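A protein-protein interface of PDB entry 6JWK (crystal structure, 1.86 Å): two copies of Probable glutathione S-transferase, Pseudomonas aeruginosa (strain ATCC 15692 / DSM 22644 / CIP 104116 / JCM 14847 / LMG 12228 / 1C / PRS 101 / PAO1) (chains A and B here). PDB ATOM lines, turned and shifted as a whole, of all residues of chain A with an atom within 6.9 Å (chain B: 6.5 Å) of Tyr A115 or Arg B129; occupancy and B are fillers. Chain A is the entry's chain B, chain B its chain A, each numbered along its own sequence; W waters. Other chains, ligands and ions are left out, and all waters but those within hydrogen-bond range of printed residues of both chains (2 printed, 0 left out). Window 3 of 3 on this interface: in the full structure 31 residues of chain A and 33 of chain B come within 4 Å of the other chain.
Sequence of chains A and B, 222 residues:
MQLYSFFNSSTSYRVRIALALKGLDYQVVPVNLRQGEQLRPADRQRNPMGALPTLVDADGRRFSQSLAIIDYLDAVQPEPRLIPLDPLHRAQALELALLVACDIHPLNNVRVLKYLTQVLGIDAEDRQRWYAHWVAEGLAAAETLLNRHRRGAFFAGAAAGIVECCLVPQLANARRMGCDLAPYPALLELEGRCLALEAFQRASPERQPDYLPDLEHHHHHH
No position is printed for both chains. Of the 7 pairs that touch across the chains among the printed residues, none has its exchanged pair printed and touching as well.
Water W2 lies within hydrogen-bond range of the backbone carbonyl oxygen (O) of Asp B126 (2.4 Å), the side-chain hydroxyl (OH) of Tyr A115 (2.7 Å) and the backbone NH (N) of Trp B130 (3.5 Å). Water W1 bridges O of Trp B134 (2.7 Å) and NH2 of Arg A111 (3.2 Å).
N of Leu A120 is in hydrogen-bond range of O of Tyr A115. N of Ile A122 is in hydrogen-bond range of O of Leu A116 (3.0 Å). The backbone carbonyl oxygen (O) of Leu A116 is in hydrogen-bond range of the backbone NH (N) of Gly A121, 3.2 Å away. The side-chain carboxylate (OE1) of Glu B125 lies within salt-bridge range of the guanidinium group (NH2) of Arg B129, 2.8 Å away.
Among the printed residues, pairs that only touch across the chains: Tyr A115 with Trp B130 (3.5 Å), Tyr A115 with Arg B129 (3.5 Å), Arg A111 with Trp B134 (3.6 Å), Tyr A115 with His B133 (3.7 Å), Tyr A115 with Trp B134 (3.8 Å), Leu A116 with Trp B130 (3.8 Å) and Val A112 with Trp B130 (3.9 Å).
Of the 13 printed residues of chain A, 4 touch a printed residue of chain B. Hydrophobic or aromatic side chains of chain B that line the printed part of chain A: Trp B130, His B133 and Trp B134. Along chain B the printed residues that touch a printed residue of chain A span positions 129 to 134.
Of the printed residues of chain B, Tyr A115 touches Arg B129, Trp B130, His B133 and Trp B134. Of chain A, only Tyr A115 (3.5 Å) comes within 4 Å of Arg B129. Of the printed residues of chain B, Leu A116 touches Trp B130 (3.8 Å). Of the printed residues of chain B, Arg A111 touches Trp B134 (3.6 Å). Printed residues of chain A within 4 Å of His B133: Tyr A115. Of the printed residues of chain A, Trp B130 touches Val A112, Tyr A115 and Leu A116. Of the printed residues of chain A, Trp B134 touches Arg A111 and Tyr A115. The nearest residue of chain A that does not touch Arg B129 is Val A119 (6.5 Å). The nearest printed residue of chain A that does not touch Trp B134 is Val A112 (4.2 Å).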
ATOM      1  N   VAL A 110     -10.592 -37.056   5.250  1.00  0.00           N
ATOM      2  CA  VAL A 110     -11.541 -36.366   4.329  1.00  0.00           C
ATOM      3  C   VAL A 110     -11.887 -34.972   4.894  1.00  0.00           C
ATOM      4  O   VAL A 110     -11.842 -34.015   4.145  1.00  0.00           O
ATOM      5  CB  VAL A 110     -12.781 -37.218   4.028  1.00  0.00           C
ATOM      6  CG1 VAL A 110     -13.474 -37.726   5.284  1.00  0.00           C
ATOM      7  CG2 VAL A 110     -13.733 -36.437   3.152  1.00  0.00           C
ATOM      8  N   ARG A 111     -12.130 -34.869   6.177  1.00  0.00           N
ATOM      9  CA  ARG A 111     -12.470 -33.614   6.785  1.00  0.00           C
ATOM     10  C   ARG A 111     -11.406 -32.540   6.473  1.00  0.00           C
ATOM     11  O   ARG A 111     -11.733 -31.466   6.063  1.00  0.00           O
ATOM     12  CB  ARG A 111     -12.841 -33.831   8.272  1.00  0.00           C
ATOM     13  CG  ARG A 111     -12.075 -33.071   9.321  1.00  0.00           C
ATOM     14  CD  ARG A 111     -12.395 -33.467  10.764  1.00  0.00           C
ATOM     15  NE  ARG A 111     -11.173 -33.616  11.530  1.00  0.00           N
ATOM     16  CZ  ARG A 111     -10.921 -33.069  12.703  1.00  0.00           C
ATOM     17  NH1 ARG A 111      -9.771 -33.291  13.264  1.00  0.00           N
ATOM     18  NH2 ARG A 111     -11.812 -32.323  13.327  1.00  0.00           N
ATOM     19  N   VAL A 112     -10.134 -32.866   6.568  1.00  0.00           N
ATOM     20  CA  VAL A 112      -9.094 -31.896   6.290  1.00  0.00           C
ATOM     21  C   VAL A 112      -8.979 -31.504   4.815  1.00  0.00           C
ATOM     22  O   VAL A 112      -8.733 -30.373   4.486  1.00  0.00           O
ATOM     23  CB  VAL A 112      -7.728 -32.384   6.794  1.00  0.00           C
ATOM     24  CG1 VAL A 112      -6.633 -31.424   6.418  1.00  0.00           C
ATOM     25  CG2 VAL A 112      -7.767 -32.578   8.285  1.00  0.00           C
ATOM     26  N   LEU A 113      -9.141 -32.484   3.952  1.00  0.00           N
ATOM     27  CA  LEU A 113      -9.038 -32.301   2.485  1.00  0.00           C
ATOM     28  C   LEU A 113     -10.237 -31.462   2.023  1.00  0.00           C
ATOM     29  O   LEU A 113     -10.020 -30.644   1.155  1.00  0.00           O
ATOM     30  CB  LEU A 113      -9.004 -33.654   1.773  1.00  0.00           C
ATOM     31  CG  LEU A 113      -7.820 -34.556   2.110  1.00  0.00           C
ATOM     32  CD1 LEU A 113      -8.033 -35.920   1.479  1.00  0.00           C
ATOM     33  CD2 LEU A 113      -6.496 -33.938   1.689  1.00  0.00           C
ATOM     34  N   LYS A 114     -11.413 -31.616   2.632  1.00  0.00           N
ATOM     35  CA  LYS A 114     -12.583 -30.733   2.356  1.00  0.00           C
ATOM     36  C   LYS A 114     -12.211 -29.307   2.749  1.00  0.00           C
ATOM     37  O   LYS A 114     -12.387 -28.399   1.902  1.00  0.00           O
ATOM     38  CB  LYS A 114     -13.835 -31.112   3.149  1.00  0.00           C
ATOM     39  CG  LYS A 114     -14.617 -32.315   2.645  1.00  0.00           C
ATOM     40  CD  LYS A 114     -15.815 -32.633   3.539  1.00  0.00           C
ATOM     41  CE  LYS A 114     -16.443 -33.991   3.297  1.00  0.00           C
ATOM     42  NZ  LYS A 114     -16.902 -34.140   1.895  1.00  0.00           N
ATOM     43  N   TYR A 115     -11.703 -29.091   3.970  1.00  0.00           N
ATOM     44  CA  TYR A 115     -11.269 -27.728   4.388  1.00  0.00           C
ATOM     45  C   TYR A 115     -10.277 -27.171   3.368  1.00  0.00           C
ATOM     46  O   TYR A 115     -10.444 -25.990   2.978  1.00  0.00           O
ATOM     47  CB  TYR A 115     -10.674 -27.670   5.797  1.00  0.00           C
ATOM     48  CG  TYR A 115     -10.505 -26.274   6.358  1.00  0.00           C
ATOM     49  CD1 TYR A 115      -9.410 -25.494   6.015  1.00  0.00           C
ATOM     50  CD2 TYR A 115     -11.409 -25.742   7.276  1.00  0.00           C
ATOM     51  CE1 TYR A 115      -9.245 -24.216   6.517  1.00  0.00           C
ATOM     52  CE2 TYR A 115     -11.239 -24.471   7.814  1.00  0.00           C
ATOM     53  CZ  TYR A 115     -10.155 -23.701   7.433  1.00  0.00           C
ATOM     54  OH  TYR A 115      -9.948 -22.439   7.933  1.00  0.00           O
ATOM     55  N   LEU A 116      -9.249 -27.931   2.970  1.00  0.00           N
ATOM     56  CA  LEU A 116      -8.211 -27.404   2.033  1.00  0.00           C
ATOM     57  C   LEU A 116      -8.903 -26.966   0.721  1.00  0.00           C
ATOM     58  O   LEU A 116      -8.534 -25.903   0.194  1.00  0.00           O
ATOM     59  CB  LEU A 116      -7.111 -28.447   1.776  1.00  0.00           C
ATOM     60  CG  LEU A 116      -6.100 -28.673   2.902  1.00  0.00           C
ATOM     61  CD1 LEU A 116      -5.111 -29.784   2.532  1.00  0.00           C
ATOM     62  CD2 LEU A 116      -5.346 -27.397   3.278  1.00  0.00           C
ATOM     63  N   THR A 117      -9.879 -27.736   0.222  1.00  0.00           N
ATOM     64  CA  THR A 117     -10.619 -27.476  -1.050  1.00  0.00           C
ATOM     65  C   THR A 117     -11.516 -26.242  -0.842  1.00  0.00           C
ATOM     66  O   THR A 117     -11.161 -25.138  -1.325  1.00  0.00           O
ATOM     67  CB  THR A 117     -11.450 -28.699  -1.476  1.00  0.00           C
ATOM     68  OG1 THR A 117     -10.635 -29.869  -1.416  1.00  0.00           O
ATOM     69  CG2 THR A 117     -12.041 -28.587  -2.867  1.00  0.00           C
ATOM     70  N   GLN A 118     -12.548 -26.419  -0.014  1.00  0.00           N
ATOM     71  CA  GLN A 118     -13.742 -25.547   0.111  1.00  0.00           C
ATOM     72  C   GLN A 118     -13.382 -24.252   0.825  1.00  0.00           C
ATOM     73  O   GLN A 118     -14.104 -23.282   0.603  1.00  0.00           O
ATOM     74  CB  GLN A 118     -14.877 -26.284   0.816  1.00  0.00           C
ATOM     75  CG  GLN A 118     -15.314 -27.498   0.017  1.00  0.00           C
ATOM     76  CD  GLN A 118     -16.486 -28.236   0.603  1.00  0.00           C
ATOM     77  OE1 GLN A 118     -16.775 -28.155   1.794  1.00  0.00           O
ATOM     78  NE2 GLN A 118     -17.153 -28.998  -0.243  1.00  0.00           N
ATOM     79  N   VAL A 119     -12.299 -24.209   1.600  1.00  0.00           N
ATOM     80  CA  VAL A 119     -11.953 -22.981   2.371  1.00  0.00           C
ATOM     81  C   VAL A 119     -10.715 -22.310   1.792  1.00  0.00           C
ATOM     82  O   VAL A 119     -10.721 -21.093   1.754  1.00  0.00           O
ATOM     83  CB  VAL A 119     -11.761 -23.235   3.879  1.00  0.00           C
ATOM     84  CG1 VAL A 119     -11.441 -21.932   4.599  1.00  0.00           C
ATOM     85  CG2 VAL A 119     -12.964 -23.945   4.494  1.00  0.00           C
ATOM     86  N   LEU A 120      -9.640 -23.044   1.490  1.00  0.00           N
ATOM     87  CA  LEU A 120      -8.371 -22.401   1.066  1.00  0.00           C
ATOM     88  C   LEU A 120      -8.200 -22.529  -0.459  1.00  0.00           C
ATOM     89  O   LEU A 120      -7.199 -22.005  -0.971  1.00  0.00           O
ATOM     90  CB  LEU A 120      -7.198 -22.974   1.864  1.00  0.00           C
ATOM     91  CG  LEU A 120      -7.228 -22.650   3.363  1.00  0.00           C
ATOM     92  CD1 LEU A 120      -6.234 -23.509   4.122  1.00  0.00           C
ATOM     93  CD2 LEU A 120      -6.958 -21.168   3.630  1.00  0.00           C
ATOM     94  N   GLY A 121      -9.181 -23.111  -1.142  1.00  0.00           N
ATOM     95  CA  GLY A 121      -9.174 -23.347  -2.604  1.00  0.00           C
ATOM     96  C   GLY A 121      -7.911 -24.033  -3.121  1.00  0.00           C
ATOM     97  O   GLY A 121      -7.393 -23.604  -4.173  1.00  0.00           O
ATOM     98  N   ILE A 122      -7.410 -25.061  -2.430  1.00  0.00           N
ATOM     99  CA  ILE A 122      -6.198 -25.838  -2.859  1.00  0.00           C
ATOM    100  C   ILE A 122      -6.658 -26.890  -3.878  1.00  0.00           C
ATOM    101  O   ILE A 122      -7.646 -27.606  -3.564  1.00  0.00           O
ATOM    102  CB  ILE A 122      -5.513 -26.479  -1.630  1.00  0.00           C
ATOM    103  CG1 ILE A 122      -5.227 -25.446  -0.533  1.00  0.00           C
ATOM    104  CG2 ILE A 122      -4.255 -27.232  -2.033  1.00  0.00           C
ATOM    105  CD1 ILE A 122      -4.281 -24.329  -0.965  1.00  0.00           C
ATOM    106  N   ALA B 124      -1.001 -15.229   7.555  1.00  0.00           N
ATOM    107  CA  ALA B 124      -1.111 -15.304   9.039  1.00  0.00           C
ATOM    108  C   ALA B 124      -2.579 -15.409   9.475  1.00  0.00           C
ATOM    109  O   ALA B 124      -2.858 -16.123  10.469  1.00  0.00           O
ATOM    110  CB  ALA B 124      -0.442 -14.106   9.678  1.00  0.00           C
ATOM    111  N   GLU B 125      -3.476 -14.742   8.755  1.00  0.00           N
ATOM    112  CA  GLU B 125      -4.904 -14.586   9.135  1.00  0.00           C
ATOM    113  C   GLU B 125      -5.695 -15.852   8.787  1.00  0.00           C
ATOM    114  O   GLU B 125      -6.621 -16.224   9.537  1.00  0.00           O
ATOM    115  CB  GLU B 125      -5.490 -13.383   8.396  1.00  0.00           C
ATOM    116  CG  GLU B 125      -6.813 -12.892   8.962  1.00  0.00           C
ATOM    117  CD  GLU B 125      -7.154 -11.444   8.624  1.00  0.00           C
ATOM    118  OE1 GLU B 125      -8.011 -11.237   7.747  1.00  0.00           O
ATOM    119  OE2 GLU B 125      -6.563 -10.525   9.242  1.00  0.00           O
ATOM    120  N   ASP B 126      -5.395 -16.445   7.636  1.00  0.00           N
ATOM    121  CA  ASP B 126      -6.008 -17.714   7.176  1.00  0.00           C
ATOM    122  C   ASP B 126      -5.511 -18.857   8.070  1.00  0.00           C
ATOM    123  O   ASP B 126      -6.305 -19.761   8.325  1.00  0.00           O
ATOM    124  CB  ASP B 126      -5.697 -17.949   5.701  1.00  0.00           C
ATOM    125  CG  ASP B 126      -6.507 -17.060   4.783  1.00  0.00           C
ATOM    126  OD1 ASP B 126      -7.725 -17.007   4.975  1.00  0.00           O
ATOM    127  OD2 ASP B 126      -5.905 -16.439   3.896  1.00  0.00           O
ATOM    128  N   ARG B 127      -4.255 -18.787   8.515  1.00  0.00           N
ATOM    129  CA  ARG B 127      -3.614 -19.757   9.432  1.00  0.00           C
ATOM    130  C   ARG B 127      -4.243 -19.653  10.820  1.00  0.00           C
ATOM    131  O   ARG B 127      -4.342 -20.708  11.454  1.00  0.00           O
ATOM    132  CB  ARG B 127      -2.105 -19.538   9.529  1.00  0.00           C
ATOM    133  CG  ARG B 127      -1.383 -19.848   8.226  1.00  0.00           C
ATOM    134  CD  ARG B 127       0.050 -20.266   8.448  1.00  0.00           C
ATOM    135  NE  ARG B 127       0.822 -19.267   9.176  1.00  0.00           N
ATOM    136  CZ  ARG B 127       1.258 -18.118   8.659  1.00  0.00           C
ATOM    137  NH1 ARG B 127       0.985 -17.801   7.400  1.00  0.00           N
ATOM    138  NH2 ARG B 127       1.962 -17.288   9.403  1.00  0.00           N
ATOM    139  N   GLN B 128      -4.592 -18.433  11.252  1.00  0.00           N
ATOM    140  CA  GLN B 128      -5.390 -18.147  12.472  1.00  0.00           C
ATOM    141  C   GLN B 128      -6.704 -18.914  12.403  1.00  0.00           C
ATOM    142  O   GLN B 128      -7.037 -19.592  13.421  1.00  0.00           O
ATOM    143  CB  GLN B 128      -5.783 -16.664  12.619  1.00  0.00           C
ATOM    144  CG  GLN B 128      -6.956 -16.425  13.598  1.00  0.00           C
ATOM    145  CD  GLN B 128      -6.467 -16.775  14.974  1.00  0.00           C
ATOM    146  OE1 GLN B 128      -5.254 -16.898  15.151  1.00  0.00           O
ATOM    147  NE2 GLN B 128      -7.371 -16.980  15.928  1.00  0.00           N
ATOM    148  N   ARG B 129      -7.473 -18.681  11.342  1.00  0.00           N
ATOM    149  CA  ARG B 129      -8.820 -19.271  11.139  1.00  0.00           C
ATOM    150  C   ARG B 129      -8.740 -20.810  11.012  1.00  0.00           C
ATOM    151  O   ARG B 129      -9.700 -21.516  11.348  1.00  0.00           O
ATOM    152  CB  ARG B 129      -9.469 -18.712   9.879  1.00  0.00           C
ATOM    153  CG  ARG B 129      -9.731 -17.211   9.935  1.00  0.00           C
ATOM    154  CD  ARG B 129     -10.312 -16.683   8.633  1.00  0.00           C
ATOM    155  NE  ARG B 129      -9.920 -15.295   8.383  1.00  0.00           N
ATOM    156  CZ  ARG B 129     -10.409 -14.219   9.022  1.00  0.00           C
ATOM    157  NH1 ARG B 129     -11.313 -14.343   9.985  1.00  0.00           N
ATOM    158  NH2 ARG B 129      -9.976 -13.007   8.708  1.00  0.00           N
ATOM    159  N   TRP B 130      -7.674 -21.321  10.422  1.00  0.00           N
ATOM    160  CA  TRP B 130      -7.455 -22.782  10.361  1.00  0.00           C
ATOM    161  C   TRP B 130      -7.311 -23.263  11.808  1.00  0.00           C
ATOM    162  O   TRP B 130      -8.104 -24.140  12.203  1.00  0.00           O
ATOM    163  CB  TRP B 130      -6.222 -23.073   9.508  1.00  0.00           C
ATOM    164  CG  TRP B 130      -5.573 -24.398   9.716  1.00  0.00           C
ATOM    165  CD1 TRP B 130      -4.724 -24.747  10.723  1.00  0.00           C
ATOM    166  CD2 TRP B 130      -5.610 -25.513   8.815  1.00  0.00           C
ATOM    167  NE1 TRP B 130      -4.246 -26.013  10.513  1.00  0.00           N
ATOM    168  CE2 TRP B 130      -4.776 -26.512   9.355  1.00  0.00           C
ATOM    169  CE3 TRP B 130      -6.264 -25.769   7.606  1.00  0.00           C
ATOM    170  CZ2 TRP B 130      -4.610 -27.761   8.749  1.00  0.00           C
ATOM    171  CZ3 TRP B 130      -6.086 -26.997   7.004  1.00  0.00           C
ATOM    172  CH2 TRP B 130      -5.295 -27.988   7.584  1.00  0.00           C
ATOM    173  N   TYR B 131      -6.353 -22.663  12.522  1.00  0.00           N
ATOM    174  CA  TYR B 131      -5.968 -22.990  13.908  1.00  0.00           C
ATOM    175  C   TYR B 131      -7.247 -22.927  14.736  1.00  0.00           C
ATOM    176  O   TYR B 131      -7.555 -23.932  15.407  1.00  0.00           O
ATOM    177  CB  TYR B 131      -4.857 -22.091  14.458  1.00  0.00           C
ATOM    178  CG  TYR B 131      -4.199 -22.641  15.695  1.00  0.00           C
ATOM    179  CD1 TYR B 131      -4.872 -22.718  16.914  1.00  0.00           C
ATOM    180  CD2 TYR B 131      -2.920 -23.153  15.644  1.00  0.00           C
ATOM    181  CE1 TYR B 131      -4.272 -23.244  18.049  1.00  0.00           C
ATOM    182  CE2 TYR B 131      -2.297 -23.656  16.777  1.00  0.00           C
ATOM    183  CZ  TYR B 131      -2.979 -23.732  17.979  1.00  0.00           C
ATOM    184  OH  TYR B 131      -2.315 -24.240  19.075  1.00  0.00           O
ATOM    185  N   ALA B 132      -8.014 -21.840  14.612  1.00  0.00           N
ATOM    186  CA  ALA B 132      -9.230 -21.626  15.424  1.00  0.00           C
ATOM    187  C   ALA B 132     -10.312 -22.650  15.062  1.00  0.00           C
ATOM    188  O   ALA B 132     -11.078 -23.096  15.969  1.00  0.00           O
ATOM    189  CB  ALA B 132      -9.712 -20.198  15.295  1.00  0.00           C
ATOM    190  N   HIS B 133     -10.448 -23.014  13.793  1.00  0.00           N
ATOM    191  CA  HIS B 133     -11.484 -23.992  13.357  1.00  0.00           C
ATOM    192  C   HIS B 133     -11.271 -25.351  14.060  1.00  0.00           C
ATOM    193  O   HIS B 133     -12.230 -25.855  14.678  1.00  0.00           O
ATOM    194  CB  HIS B 133     -11.479 -24.165  11.825  1.00  0.00           C
ATOM    195  CG  HIS B 133     -12.456 -25.185  11.342  1.00  0.00           C
ATOM    196  ND1 HIS B 133     -13.814 -24.967  11.377  1.00  0.00           N
ATOM    197  CD2 HIS B 133     -12.293 -26.428  10.833  1.00  0.00           C
ATOM    198  CE1 HIS B 133     -14.454 -26.034  10.906  1.00  0.00           C
ATOM    199  NE2 HIS B 133     -13.544 -26.944  10.576  1.00  0.00           N
ATOM    200  N   TRP B 134     -10.061 -25.919  14.033  1.00  0.00           N
ATOM    201  CA  TRP B 134      -9.850 -27.286  14.603  1.00  0.00           C
ATOM    202  C   TRP B 134      -9.972 -27.218  16.133  1.00  0.00           C
ATOM    203  O   TRP B 134     -10.464 -28.185  16.678  1.00  0.00           O
ATOM    204  CB  TRP B 134      -8.522 -27.918  14.123  1.00  0.00           C
ATOM    205  CG  TRP B 134      -8.396 -27.897  12.623  1.00  0.00           C
ATOM    206  CD1 TRP B 134      -7.481 -27.215  11.880  1.00  0.00           C
ATOM    207  CD2 TRP B 134      -9.281 -28.518  11.680  1.00  0.00           C
ATOM    208  NE1 TRP B 134      -7.738 -27.371  10.545  1.00  0.00           N
ATOM    209  CE2 TRP B 134      -8.835 -28.161  10.390  1.00  0.00           C
ATOM    210  CE3 TRP B 134     -10.388 -29.366  11.790  1.00  0.00           C
ATOM    211  CZ2 TRP B 134      -9.443 -28.634   9.238  1.00  0.00           C
ATOM    212  CZ3 TRP B 134     -11.015 -29.799  10.650  1.00  0.00           C
ATOM    213  CH2 TRP B 134     -10.529 -29.461   9.389  1.00  0.00           C
HETATM  214  O   HOH W   1     -10.700 -30.713  15.799  1.00  0.00           O
HETATM  215  O   HOH W   2      -8.062 -20.753   7.019  1.00  0.00           O
